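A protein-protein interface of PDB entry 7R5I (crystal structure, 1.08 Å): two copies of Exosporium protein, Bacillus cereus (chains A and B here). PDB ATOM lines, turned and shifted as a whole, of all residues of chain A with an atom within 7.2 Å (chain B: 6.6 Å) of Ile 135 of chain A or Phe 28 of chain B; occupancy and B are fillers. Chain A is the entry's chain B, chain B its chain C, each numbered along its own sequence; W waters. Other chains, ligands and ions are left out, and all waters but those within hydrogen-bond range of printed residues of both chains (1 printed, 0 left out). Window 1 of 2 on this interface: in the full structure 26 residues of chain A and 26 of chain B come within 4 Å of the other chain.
Of the 20 printed residues of chain A, 6 touch a printed residue of chain B.
Hydrophobic or aromatic side chains of chain A that line the printed part of chain B: Ile 77, Pro 112, Ile 135 and Leu 136.
Along chain A the printed residues that touch a printed residue of chain B span positions 77 to 136.
Hydrophobic or aromatic side chains of chain B that line the printed part of chain A: Phe 26, Phe 28, Phe 30, Pro 51 and Val 59.
Among the printed residues, 13 pairs touch across the chains.
Among the printed residues, no Asp or Glu carboxylate lies within 4 Å of a Lys or Arg side-chain nitrogen of the other chain.
Among the printed residues, pairs that only touch across the chains: Pro 112 of chain A with Pro 51 of chain B, Leu 136 of chain A with Pro 51 of chain B, Gly 113 of chain A with Thr 83 of chain B, Leu 136 of chain A with Val 165 of chain B, Leu 136 of chain A with Thr 164 of chain B, Leu 136 of chain A with Gly 27 of chain B, Leu 136 of chain A with Val 59 of chain B, Ile 77 of chain A with Phe 26 of chain B, Pro 112 of chain A with Phe 30 of chain B, Leu 136 of chain A with Phe 28 of chain B, Val 134 of chain A with Phe 28 of chain B and Ile 135 of chain A with Phe 28 of chain B.
1 position is printed for both chains.
N of Gly 27 of chain B is in hydrogen-bond range of O of Val 165 of chain B (2.9 Å).
The backbone carbonyl oxygen (O) of Thr 83 of chain B lies within hydrogen-bond range of the backbone NH (N) of Ala 162 of chain B.
O of Phe 26 of chain B is in hydrogen-bond range of OG1 of Thr 63 of chain B, 2.9 Å away.
The backbone carbonyl oxygen (O) of Val 59 of chain B is in hydrogen-bond range of the backbone NH (N) of Phe 28 of chain B (3.0 Å).
The backbone NH (N) of Val 59 of chain B sits at hydrogen-bond distance from the backbone carbonyl oxygen (O) of Val 49 of chain B, at 2.8 Å.
O of Ile 80 of chain A lies within hydrogen-bond range of N of Ile 135 of chain A, 2.9 Å away.
The backbone carbonyl oxygen of Val 134 of chain A sits at hydrogen-bond distance from the side-chain hydroxyl of Thr 164 of chain B.
Water W1 bridges the backbone carbonyl oxygen (O) of Gly 115 of chain A and the side-chain hydroxyl (OG1) of Thr 83 of chain B.
Leu 102 of chain A touches none of the printed residues of chain B.
Of the printed residues of chain B, Gly 113 of chain A touches Thr 83 (3.5 Å).
Printed residues of chain B within 4 Å of Val 134 of chain A: Phe 28 and Thr 164.
Of the printed residues of chain B, Ile 135 of chain A touches Phe 28.
Printed residues of chain B within 4 Å of Leu 136 of chain A: Gly 27, Phe 28, Pro 51, Val 59, Thr 164 and Val 165.
Of the printed residues of chain A, Phe 26 of chain B touches Ile 77 (3.7 Å).
Of the printed residues of chain A, Phe 28 of chain B touches Val 134 (3.8 Å), Ile 135 (3.9 Å) and Leu 136 (3.8 Å).
Ala 29 of chain B touches none of the printed residues of chain A.
Of the printed residues of chain A, Thr 83 of chain B touches Gly 113.
The nearest printed residue of chain B that does not touch Ile 135 of chain A is Thr 164 of chain B (4.7 Å).
The nearest printed residue of chain B that does not touch Leu 136 of chain A is Phe 26 of chain B (4.1 Å).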
ATOM      1  N   ILE A  77      16.226   1.938  13.242  1.00  0.00           N
ATOM      2  CA  ILE A  77      17.103   1.874  14.429  1.00  0.00           C
ATOM      3  C   ILE A  77      16.689   0.620  15.216  1.00  0.00           C
ATOM      4  O   ILE A  77      15.469   0.475  15.453  1.00  0.00           O
ATOM      5  CB  ILE A  77      16.971   3.133  15.288  1.00  0.00           C
ATOM      6  CG1 ILE A  77      17.248   4.399  14.466  1.00  0.00           C
ATOM      7  CG2 ILE A  77      17.852   3.048  16.543  1.00  0.00           C
ATOM      8  CD1 ILE A  77      18.618   4.538  13.939  1.00  0.00           C
ATOM      9  N   TYR A  78      17.635  -0.214  15.505  1.00  0.00           N
ATOM     10  CA  TYR A  78      17.399  -1.490  16.206  1.00  0.00           C
ATOM     11  C   TYR A  78      18.144  -1.537  17.510  1.00  0.00           C
ATOM     12  O   TYR A  78      19.218  -0.973  17.633  1.00  0.00           O
ATOM     13  CB  TYR A  78      17.874  -2.626  15.288  1.00  0.00           C
ATOM     14  CG  TYR A  78      17.003  -2.837  14.074  1.00  0.00           C
ATOM     15  CD1 TYR A  78      17.119  -2.068  12.944  1.00  0.00           C
ATOM     16  CD2 TYR A  78      16.052  -3.858  14.086  1.00  0.00           C
ATOM     17  CE1 TYR A  78      16.280  -2.268  11.845  1.00  0.00           C
ATOM     18  CE2 TYR A  78      15.228  -4.073  12.996  1.00  0.00           C
ATOM     19  CZ  TYR A  78      15.366  -3.279  11.866  1.00  0.00           C
ATOM     20  OH  TYR A  78      14.527  -3.527  10.820  1.00  0.00           O
ATOM     21  N   GLN A  79      17.565  -2.281  18.449  1.00  0.00           N
ATOM     22  CA  GLN A  79      18.302  -2.793  19.579  1.00  0.00           C
ATOM     23  C   GLN A  79      18.816  -4.189  19.256  1.00  0.00           C
ATOM     24  O   GLN A  79      17.969  -5.058  18.833  1.00  0.00           O
ATOM     25  CB  GLN A  79      17.551  -2.745  20.898  1.00  0.00           C
ATOM     26  CG  GLN A  79      16.222  -3.501  20.887  1.00  0.00           C
ATOM     27  CD  GLN A  79      15.771  -3.771  22.287  1.00  0.00           C
ATOM     28  OE1 GLN A  79      14.862  -3.074  22.753  1.00  0.00           O
ATOM     29  NE2 GLN A  79      16.433  -4.597  22.998  1.00  0.00           N
ATOM     30  N   ILE A  80      20.064  -4.499  19.451  1.00  0.00           N
ATOM     31  CA  ILE A  80      20.663  -5.795  19.258  1.00  0.00           C
ATOM     32  C   ILE A  80      21.419  -6.181  20.522  1.00  0.00           C
ATOM     33  O   ILE A  80      22.069  -5.366  21.162  1.00  0.00           O
ATOM     34  CB  ILE A  80      21.462  -5.867  17.944  1.00  0.00           C
ATOM     35  CG1 ILE A  80      22.735  -5.007  18.003  1.00  0.00           C
ATOM     36  CG2 ILE A  80      20.618  -5.529  16.743  1.00  0.00           C
ATOM     37  CD1 ILE A  80      23.599  -5.077  16.757  1.00  0.00           C
ATOM     38  N   SER A  81      21.414  -7.479  20.837  1.00  0.00           N
ATOM     39  CA  SER A  81      22.066  -8.011  22.029  1.00  0.00           C
ATOM     40  C   SER A  81      22.087  -9.525  21.935  1.00  0.00           C
ATOM     41  O   SER A  81      21.407 -10.118  21.099  1.00  0.00           O
ATOM     42  CB  SER A  81      21.308  -7.574  23.296  1.00  0.00           C
ATOM     43  OG  SER A  81      19.977  -8.070  23.319  1.00  0.00           O
ATOM     44  N   TYR A  82      22.862 -10.159  22.811  1.00  0.00           N
ATOM     45  CA  TYR A  82      22.960 -11.607  22.788  1.00  0.00           C
ATOM     46  C   TYR A  82      23.352 -12.148  24.145  1.00  0.00           C
ATOM     47  O   TYR A  82      23.827 -11.434  25.029  1.00  0.00           O
ATOM     48  CB  TYR A  82      23.928 -12.097  21.698  1.00  0.00           C
ATOM     49  CG  TYR A  82      25.347 -11.730  21.970  1.00  0.00           C
ATOM     50  CD1 TYR A  82      25.829 -10.463  21.647  1.00  0.00           C
ATOM     51  CD2 TYR A  82      26.245 -12.641  22.472  1.00  0.00           C
ATOM     52  CE1 TYR A  82      27.159 -10.122  21.863  1.00  0.00           C
ATOM     53  CE2 TYR A  82      27.558 -12.291  22.736  1.00  0.00           C
ATOM     54  CZ  TYR A  82      28.049 -11.022  22.404  1.00  0.00           C
ATOM     55  OH  TYR A  82      29.362 -10.713  22.628  1.00  0.00           O
ATOM     56  N   LEU A 102      29.207  -8.983  18.466  1.00  0.00           N
ATOM     57  CA  LEU A 102      28.346  -9.007  17.269  1.00  0.00           C
ATOM     58  C   LEU A 102      29.106  -8.443  16.077  1.00  0.00           C
ATOM     59  O   LEU A 102      29.886  -7.483  16.223  1.00  0.00           O
ATOM     60  CB  LEU A 102      27.093  -8.180  17.494  1.00  0.00           C
ATOM     61  CG  LEU A 102      26.159  -8.736  18.570  1.00  0.00           C
ATOM     62  CD1 LEU A 102      25.027  -7.859  18.805  1.00  0.00           C
ATOM     63  CD2 LEU A 102      25.693 -10.119  18.228  1.00  0.00           C
ATOM     64  N   ILE A 111      30.954  -4.832  16.011  1.00  0.00           N
ATOM     65  CA  ILE A 111      30.151  -3.680  16.405  1.00  0.00           C
ATOM     66  C   ILE A 111      30.588  -3.204  17.774  1.00  0.00           C
ATOM     67  O   ILE A 111      30.532  -3.979  18.749  1.00  0.00           O
ATOM     68  CB  ILE A 111      28.666  -4.018  16.332  1.00  0.00           C
ATOM     69  CG1 ILE A 111      28.266  -4.446  14.915  1.00  0.00           C
ATOM     70  CG2 ILE A 111      27.830  -2.892  16.845  1.00  0.00           C
ATOM     71  CD1 ILE A 111      26.883  -5.056  14.806  1.00  0.00           C
ATOM     72  N   PRO A 112      30.935  -1.933  17.958  1.00  0.00           N
ATOM     73  CA  PRO A 112      31.327  -1.485  19.297  1.00  0.00           C
ATOM     74  C   PRO A 112      30.170  -1.619  20.276  1.00  0.00           C
ATOM     75  O   PRO A 112      29.019  -1.492  19.948  1.00  0.00           O
ATOM     76  CB  PRO A 112      31.731  -0.023  19.092  1.00  0.00           C
ATOM     77  CG  PRO A 112      31.168   0.374  17.829  1.00  0.00           C
ATOM     78  CD  PRO A 112      31.005  -0.840  16.965  1.00  0.00           C
ATOM     79  N   GLY A 113      30.551  -1.878  21.537  1.00  0.00           N
ATOM     80  CA  GLY A 113      29.585  -2.069  22.627  1.00  0.00           C
ATOM     81  C   GLY A 113      28.999  -3.455  22.722  1.00  0.00           C
ATOM     82  O   GLY A 113      28.205  -3.674  23.669  1.00  0.00           O
ATOM     83  N   SER A 114      29.421  -4.379  21.896  1.00  0.00           N
ATOM     84  CA  SER A 114      28.823  -5.725  21.856  1.00  0.00           C
ATOM     85  C   SER A 114      29.732  -6.807  22.405  1.00  0.00           C
ATOM     86  O   SER A 114      29.427  -7.984  22.212  1.00  0.00           O
ATOM     87  CB  SER A 114      28.387  -6.049  20.451  1.00  0.00           C
ATOM     88  OG  SER A 114      29.473  -6.307  19.553  1.00  0.00           O
ATOM     89  N   GLY A 115      30.787  -6.441  23.117  1.00  0.00           N
ATOM     90  CA  GLY A 115      31.706  -7.449  23.639  1.00  0.00           C
ATOM     91  C   GLY A 115      31.139  -8.207  24.849  1.00  0.00           C
ATOM     92  O   GLY A 115      30.406  -7.612  25.683  1.00  0.00           O
ATOM     93  N   SER A 132      25.420  -9.752  26.750  1.00  0.00           N
ATOM     94  CA  SER A 132      25.942  -8.491  26.247  1.00  0.00           C
ATOM     95  C   SER A 132      25.129  -7.317  26.760  1.00  0.00           C
ATOM     96  O   SER A 132      24.065  -7.464  27.374  1.00  0.00           O
ATOM     97  CB  SER A 132      25.898  -8.506  24.728  1.00  0.00           C
ATOM     98  OG  SER A 132      24.600  -8.308  24.221  1.00  0.00           O
ATOM     99  N   GLY A 133      25.653  -6.117  26.485  1.00  0.00           N
ATOM    100  CA  GLY A 133      24.810  -4.976  26.529  1.00  0.00           C
ATOM    101  C   GLY A 133      23.838  -4.897  25.355  1.00  0.00           C
ATOM    102  O   GLY A 133      23.883  -5.760  24.448  1.00  0.00           O
ATOM    103  N   VAL A 134      23.005  -3.905  25.424  1.00  0.00           N
ATOM    104  CA  VAL A 134      22.048  -3.612  24.354  1.00  0.00           C
ATOM    105  C   VAL A 134      22.625  -2.505  23.488  1.00  0.00           C
ATOM    106  O   VAL A 134      22.991  -1.447  23.993  1.00  0.00           O
ATOM    107  CB  VAL A 134      20.688  -3.191  24.911  1.00  0.00           C
ATOM    108  CG1 VAL A 134      19.715  -2.888  23.791  1.00  0.00           C
ATOM    109  CG2 VAL A 134      20.128  -4.288  25.825  1.00  0.00           C
ATOM    110  N   ILE A 135      22.830  -2.761  22.213  1.00  0.00           N
ATOM    111  CA  ILE A 135      23.431  -1.777  21.284  1.00  0.00           C
ATOM    112  C   ILE A 135      22.287  -1.199  20.469  1.00  0.00           C
ATOM    113  O   ILE A 135      21.499  -1.972  19.880  1.00  0.00           O
ATOM    114  CB  ILE A 135      24.492  -2.411  20.373  1.00  0.00           C
ATOM    115  CG1 ILE A 135      25.629  -3.035  21.175  1.00  0.00           C
ATOM    116  CG2 ILE A 135      24.969  -1.359  19.357  1.00  0.00           C
ATOM    117  CD1 ILE A 135      25.363  -4.468  21.593  1.00  0.00           C
ATOM    118  N   LEU A 136      22.206   0.121  20.374  1.00  0.00           N
ATOM    119  CA  LEU A 136      21.251   0.794  19.477  1.00  0.00           C
ATOM    120  C   LEU A 136      22.032   1.136  18.225  1.00  0.00           C
ATOM    121  O   LEU A 136      23.089   1.768  18.307  1.00  0.00           O
ATOM    122  CB  LEU A 136      20.584   2.055  20.019  1.00  0.00           C
ATOM    123  CG  LEU A 136      19.965   1.926  21.368  1.00  0.00           C
ATOM    124  CD1 LEU A 136      19.349   3.235  21.769  1.00  0.00           C
ATOM    125  CD2 LEU A 136      18.953   0.821  21.417  1.00  0.00           C
ATOM    126  N   ILE A 137      21.497   0.788  17.068  1.00  0.00           N
ATOM    127  CA  ILE A 137      22.263   0.934  15.810  1.00  0.00           C
ATOM    128  C   ILE A 137      21.289   1.104  14.658  1.00  0.00           C
ATOM    129  O   ILE A 137      20.262   0.417  14.563  1.00  0.00           O
ATOM    130  CB  ILE A 137      23.238  -0.243  15.644  1.00  0.00           C
ATOM    131  CG1 ILE A 137      24.098  -0.103  14.401  1.00  0.00           C
ATOM    132  CG2 ILE A 137      22.514  -1.588  15.680  1.00  0.00           C
ATOM    133  CD1 ILE A 137      25.283  -1.023  14.327  1.00  0.00           C
ATOM    134  N   THR A 164      19.115 -11.396  19.902  1.00  0.00           N
ATOM    135  CA  THR A 164      17.942 -10.585  19.988  1.00  0.00           C
ATOM    136  C   THR A 164      18.042  -9.346  19.110  1.00  0.00           C
ATOM    137  O   THR A 164      18.988  -8.563  19.287  1.00  0.00           O
ATOM    138  CB  THR A 164      17.687 -10.147  21.438  1.00  0.00           C
ATOM    139  OG1 THR A 164      17.558 -11.338  22.191  1.00  0.00           O
ATOM    140  CG2 THR A 164      16.503  -9.243  21.577  1.00  0.00           C
ATOM    141  N   ALA A 166      15.469  -6.161  17.680  1.00  0.00           N
ATOM    142  CA  ALA A 166      14.152  -5.525  17.693  1.00  0.00           C
ATOM    143  C   ALA A 166      14.230  -4.101  17.219  1.00  0.00           C
ATOM    144  O   ALA A 166      15.060  -3.339  17.711  1.00  0.00           O
ATOM    145  CB  ALA A 166      13.500  -5.633  19.060  1.00  0.00           C
ATOM    146  N   PHE B  26      15.829   8.542  21.827  1.00  0.00           N
ATOM    147  CA  PHE B  26      16.841   7.545  22.112  1.00  0.00           C
ATOM    148  C   PHE B  26      18.216   8.155  22.096  1.00  0.00           C
ATOM    149  O   PHE B  26      18.437   9.229  21.439  1.00  0.00           O
ATOM    150  CB  PHE B  26      16.721   6.305  21.202  1.00  0.00           C
ATOM    151  CG  PHE B  26      16.816   6.596  19.725  1.00  0.00           C
ATOM    152  CD1 PHE B  26      18.018   6.825  19.075  1.00  0.00           C
ATOM    153  CD2 PHE B  26      15.651   6.637  18.980  1.00  0.00           C
ATOM    154  CE1 PHE B  26      18.051   7.114  17.710  1.00  0.00           C
ATOM    155  CE2 PHE B  26      15.668   6.940  17.611  1.00  0.00           C
ATOM    156  CZ  PHE B  26      16.888   7.149  16.987  1.00  0.00           C
ATOM    157  N   GLY B  27      19.173   7.460  22.625  1.00  0.00           N
ATOM    158  CA  GLY B  27      20.564   7.796  22.500  1.00  0.00           C
ATOM    159  C   GLY B  27      21.451   6.628  22.806  1.00  0.00           C
ATOM    160  O   GLY B  27      21.122   5.813  23.742  1.00  0.00           O
ATOM    161  N   PHE B  28      22.569   6.519  22.142  1.00  0.00           N
ATOM    162  CA  PHE B  28      23.603   5.535  22.368  1.00  0.00           C
ATOM    163  C   PHE B  28      24.940   6.227  22.432  1.00  0.00           C
ATOM    164  O   PHE B  28      25.281   6.871  21.436  1.00  0.00           O
ATOM    165  CB  PHE B  28      23.561   4.439  21.304  1.00  0.00           C
ATOM    166  CG  PHE B  28      24.532   3.316  21.528  1.00  0.00           C
ATOM    167  CD1 PHE B  28      24.276   2.382  22.549  1.00  0.00           C
ATOM    168  CD2 PHE B  28      25.713   3.177  20.817  1.00  0.00           C
ATOM    169  CE1 PHE B  28      25.164   1.367  22.766  1.00  0.00           C
ATOM    170  CE2 PHE B  28      26.586   2.137  21.023  1.00  0.00           C
ATOM    171  CZ  PHE B  28      26.309   1.207  22.034  1.00  0.00           C
ATOM    172  N   ALA B  29      25.580   6.226  23.575  1.00  0.00           N
ATOM    173  CA  ALA B  29      26.823   6.956  23.802  1.00  0.00           C
ATOM    174  C   ALA B  29      27.861   5.968  24.232  1.00  0.00           C
ATOM    175  O   ALA B  29      27.597   5.181  25.171  1.00  0.00           O
ATOM    176  CB  ALA B  29      26.699   8.064  24.775  1.00  0.00           C
ATOM    177  N   PHE B  30      29.054   5.960  23.658  1.00  0.00           N
ATOM    178  CA  PHE B  30      30.027   4.926  23.939  1.00  0.00           C
ATOM    179  C   PHE B  30      31.443   5.459  23.906  1.00  0.00           C
ATOM    180  O   PHE B  30      31.747   6.544  23.351  1.00  0.00           O
ATOM    181  CB  PHE B  30      29.807   3.701  23.067  1.00  0.00           C
ATOM    182  CG  PHE B  30      30.127   3.890  21.597  1.00  0.00           C
ATOM    183  CD1 PHE B  30      29.183   4.437  20.760  1.00  0.00           C
ATOM    184  CD2 PHE B  30      31.350   3.484  21.093  1.00  0.00           C
ATOM    185  CE1 PHE B  30      29.472   4.609  19.390  1.00  0.00           C
ATOM    186  CE2 PHE B  30      31.647   3.672  19.726  1.00  0.00           C
ATOM    187  CZ  PHE B  30      30.681   4.199  18.903  1.00  0.00           C
ATOM    188  N   SER B  48      31.421   9.065  21.888  1.00  0.00           N
ATOM    189  CA  SER B  48      31.000   8.599  20.489  1.00  0.00           C
ATOM    190  C   SER B  48      29.546   8.319  20.554  1.00  0.00           C
ATOM    191  O   SER B  48      29.034   7.794  21.537  1.00  0.00           O
ATOM    192  CB  SER B  48      31.786   7.417  20.089  1.00  0.00           C
ATOM    193  OG  SER B  48      33.195   7.674  20.152  1.00  0.00           O
ATOM    194  N   VAL B  49      28.875   8.503  19.425  1.00  0.00           N
ATOM    195  CA  VAL B  49      27.439   8.234  19.252  1.00  0.00           C
ATOM    196  C   VAL B  49      27.136   7.454  17.973  1.00  0.00           C
ATOM    197  O   VAL B  49      25.947   7.261  17.705  1.00  0.00           O
ATOM    198  CB  VAL B  49      26.580   9.495  19.367  1.00  0.00           C
ATOM    199  CG1 VAL B  49      26.712  10.099  20.753  1.00  0.00           C
ATOM    200  CG2 VAL B  49      26.935  10.498  18.277  1.00  0.00           C
ATOM    201  N   SER B  50      28.131   6.997  17.233  1.00  0.00           N
ATOM    202  CA  SER B  50      27.913   6.457  15.874  1.00  0.00           C
ATOM    203  C   SER B  50      28.540   5.093  15.744  1.00  0.00           C
ATOM    204  O   SER B  50      29.685   4.916  15.347  1.00  0.00           O
ATOM    205  CB  SER B  50      28.491   7.411  14.821  1.00  0.00           C
ATOM    206  OG  SER B  50      27.911   8.698  14.967  1.00  0.00           O
ATOM    207  N   PRO B  51      27.767   4.011  16.124  1.00  0.00           N
ATOM    208  CA  PRO B  51      28.396   2.690  16.201  1.00  0.00           C
ATOM    209  C   PRO B  51      28.498   1.863  14.912  1.00  0.00           C
ATOM    210  O   PRO B  51      29.202   0.879  14.881  1.00  0.00           O
ATOM    211  CB  PRO B  51      27.471   1.946  17.170  1.00  0.00           C
ATOM    212  CG  PRO B  51      26.132   2.589  16.953  1.00  0.00           C
ATOM    213  CD  PRO B  51      26.437   4.055  16.740  1.00  0.00           C
ATOM    214  N   PRO B  58      24.926   9.332  13.767  1.00  0.00           N
ATOM    215  CA  PRO B  58      24.723   9.455  15.211  1.00  0.00           C
ATOM    216  C   PRO B  58      23.392   8.825  15.583  1.00  0.00           C
ATOM    217  O   PRO B  58      22.350   9.169  15.075  1.00  0.00           O
ATOM    218  CB  PRO B  58      24.685  10.960  15.450  1.00  0.00           C
ATOM    219  CG  PRO B  58      24.659  11.596  14.140  1.00  0.00           C
ATOM    220  CD  PRO B  58      25.036  10.615  13.092  1.00  0.00           C
ATOM    221  N   VAL B  59      23.452   7.949  16.581  1.00  0.00           N
ATOM    222  CA  VAL B  59      22.232   7.222  17.047  1.00  0.00           C
ATOM    223  C   VAL B  59      21.693   8.034  18.226  1.00  0.00           C
ATOM    224  O   VAL B  59      21.805   7.638  19.424  1.00  0.00           O
ATOM    225  CB  VAL B  59      22.547   5.749  17.322  1.00  0.00           C
ATOM    226  CG1 VAL B  59      21.317   5.018  17.854  1.00  0.00           C
ATOM    227  CG2 VAL B  59      23.027   5.084  16.019  1.00  0.00           C
ATOM    228  N   ILE B  60      21.107   9.167  17.918  1.00  0.00           N
ATOM    229  CA  ILE B  60      20.640  10.198  18.838  1.00  0.00           C
ATOM    230  C   ILE B  60      19.369  10.758  18.274  1.00  0.00           C
ATOM    231  O   ILE B  60      19.392  11.238  17.098  1.00  0.00           O
ATOM    232  CB  ILE B  60      21.687  11.325  19.052  1.00  0.00           C
ATOM    233  CG1 ILE B  60      23.016  10.819  19.622  1.00  0.00           C
ATOM    234  CG2 ILE B  60      21.109  12.506  19.813  1.00  0.00           C
ATOM    235  CD1 ILE B  60      22.965  10.434  21.098  1.00  0.00           C
ATOM    236  N   THR B  63      17.549  13.319  22.441  1.00  0.00           N
ATOM    237  CA  THR B  63      18.346  13.297  23.675  1.00  0.00           C
ATOM    238  C   THR B  63      19.614  14.067  23.374  1.00  0.00           C
ATOM    239  O   THR B  63      19.870  14.398  22.163  1.00  0.00           O
ATOM    240  CB  THR B  63      18.708  11.860  24.085  1.00  0.00           C
ATOM    241  OG1 THR B  63      19.575  11.249  23.140  1.00  0.00           O
ATOM    242  CG2 THR B  63      17.494  10.994  24.315  1.00  0.00           C
ATOM    243  N   SER B  65      23.842  13.800  23.990  1.00  0.00           N
ATOM    244  CA  SER B  65      25.043  13.148  24.499  1.00  0.00           C
ATOM    245  C   SER B  65      25.975  14.229  25.030  1.00  0.00           C
ATOM    246  O   SER B  65      26.512  14.974  24.176  1.00  0.00           O
ATOM    247  CB  SER B  65      25.719  12.261  23.541  1.00  0.00           C
ATOM    248  OG  SER B  65      26.865  11.612  24.098  1.00  0.00           O
ATOM    249  N   ILE B  70      23.880  10.896  29.002  1.00  0.00           N
ATOM    250  CA  ILE B  70      22.778  11.241  28.118  1.00  0.00           C
ATOM    251  C   ILE B  70      21.764  12.061  28.854  1.00  0.00           C
ATOM    252  O   ILE B  70      21.253  11.627  29.936  1.00  0.00           O
ATOM    253  CB  ILE B  70      22.171  10.006  27.424  1.00  0.00           C
ATOM    254  CG1 ILE B  70      23.205   9.383  26.480  1.00  0.00           C
ATOM    255  CG2 ILE B  70      20.876  10.358  26.743  1.00  0.00           C
ATOM    256  CD1 ILE B  70      22.814   8.036  25.915  1.00  0.00           C
ATOM    257  N   THR B  83      27.135  -1.155  29.507  1.00  0.00           N
ATOM    258  CA  THR B  83      28.134  -2.198  29.552  1.00  0.00           C
ATOM    259  C   THR B  83      29.520  -1.582  29.648  1.00  0.00           C
ATOM    260  O   THR B  83      29.719  -0.494  29.096  1.00  0.00           O
ATOM    261  CB  THR B  83      27.972  -3.150  28.352  1.00  0.00           C
ATOM    262  OG1 THR B  83      28.932  -4.205  28.448  1.00  0.00           O
ATOM    263  CG2 THR B  83      28.137  -2.507  26.984  1.00  0.00           C
ATOM    264  N   ALA B 161      33.286   1.564  27.302  1.00  0.00           N
ATOM    265  CA  ALA B 161      31.990   1.697  28.001  1.00  0.00           C
ATOM    266  C   ALA B 161      30.912   2.057  26.983  1.00  0.00           C
ATOM    267  O   ALA B 161      31.256   2.624  25.930  1.00  0.00           O
ATOM    268  CB  ALA B 161      32.094   2.749  29.077  1.00  0.00           C
ATOM    269  N   ALA B 162      29.657   1.730  27.284  1.00  0.00           N
ATOM    270  CA  ALA B 162      28.553   2.130  26.396  1.00  0.00           C
ATOM    271  C   ALA B 162      27.303   2.321  27.218  1.00  0.00           C
ATOM    272  O   ALA B 162      27.099   1.553  28.212  1.00  0.00           O
ATOM    273  CB  ALA B 162      28.287   1.124  25.280  1.00  0.00           C
ATOM    274  N   LEU B 163      26.475   3.270  26.925  1.00  0.00           N
ATOM    275  CA  LEU B 163      25.238   3.662  27.588  1.00  0.00           C
ATOM    276  C   LEU B 163      24.106   3.684  26.580  1.00  0.00           C
ATOM    277  O   LEU B 163      24.242   4.337  25.529  1.00  0.00           O
ATOM    278  CB  LEU B 163      25.430   5.010  28.246  1.00  0.00           C
ATOM    279  CG  LEU B 163      24.197   5.593  28.916  1.00  0.00           C
ATOM    280  CD1 LEU B 163      23.766   4.735  30.097  1.00  0.00           C
ATOM    281  CD2 LEU B 163      24.475   7.023  29.368  1.00  0.00           C
ATOM    282  N   THR B 164      23.011   3.036  26.913  1.00  0.00           N
ATOM    283  CA  THR B 164      21.855   2.861  26.065  1.00  0.00           C
ATOM    284  C   THR B 164      20.617   3.466  26.675  1.00  0.00           C
ATOM    285  O   THR B 164      20.243   3.013  27.808  1.00  0.00           O
ATOM    286  CB  THR B 164      21.650   1.403  25.739  1.00  0.00           C
ATOM    287  OG1 THR B 164      22.842   0.903  25.132  1.00  0.00           O
ATOM    288  CG2 THR B 164      20.439   1.143  24.895  1.00  0.00           C
ATOM    289  N   VAL B 165      19.951   4.393  26.033  1.00  0.00           N
ATOM    290  CA  VAL B 165      18.724   5.044  26.475  1.00  0.00           C
ATOM    291  C   VAL B 165      17.699   4.959  25.361  1.00  0.00           C
ATOM    292  O   VAL B 165      17.987   5.445  24.257  1.00  0.00           O
ATOM    293  CB  VAL B 165      18.989   6.484  26.884  1.00  0.00           C
ATOM    294  CG1 VAL B 165      17.727   7.228  27.171  1.00  0.00           C
ATOM    295  CG2 VAL B 165      19.978   6.574  28.052  1.00  0.00           C
HETATM  296  O   HOH W   1      28.966  -6.976  27.996  1.00  0.00           O
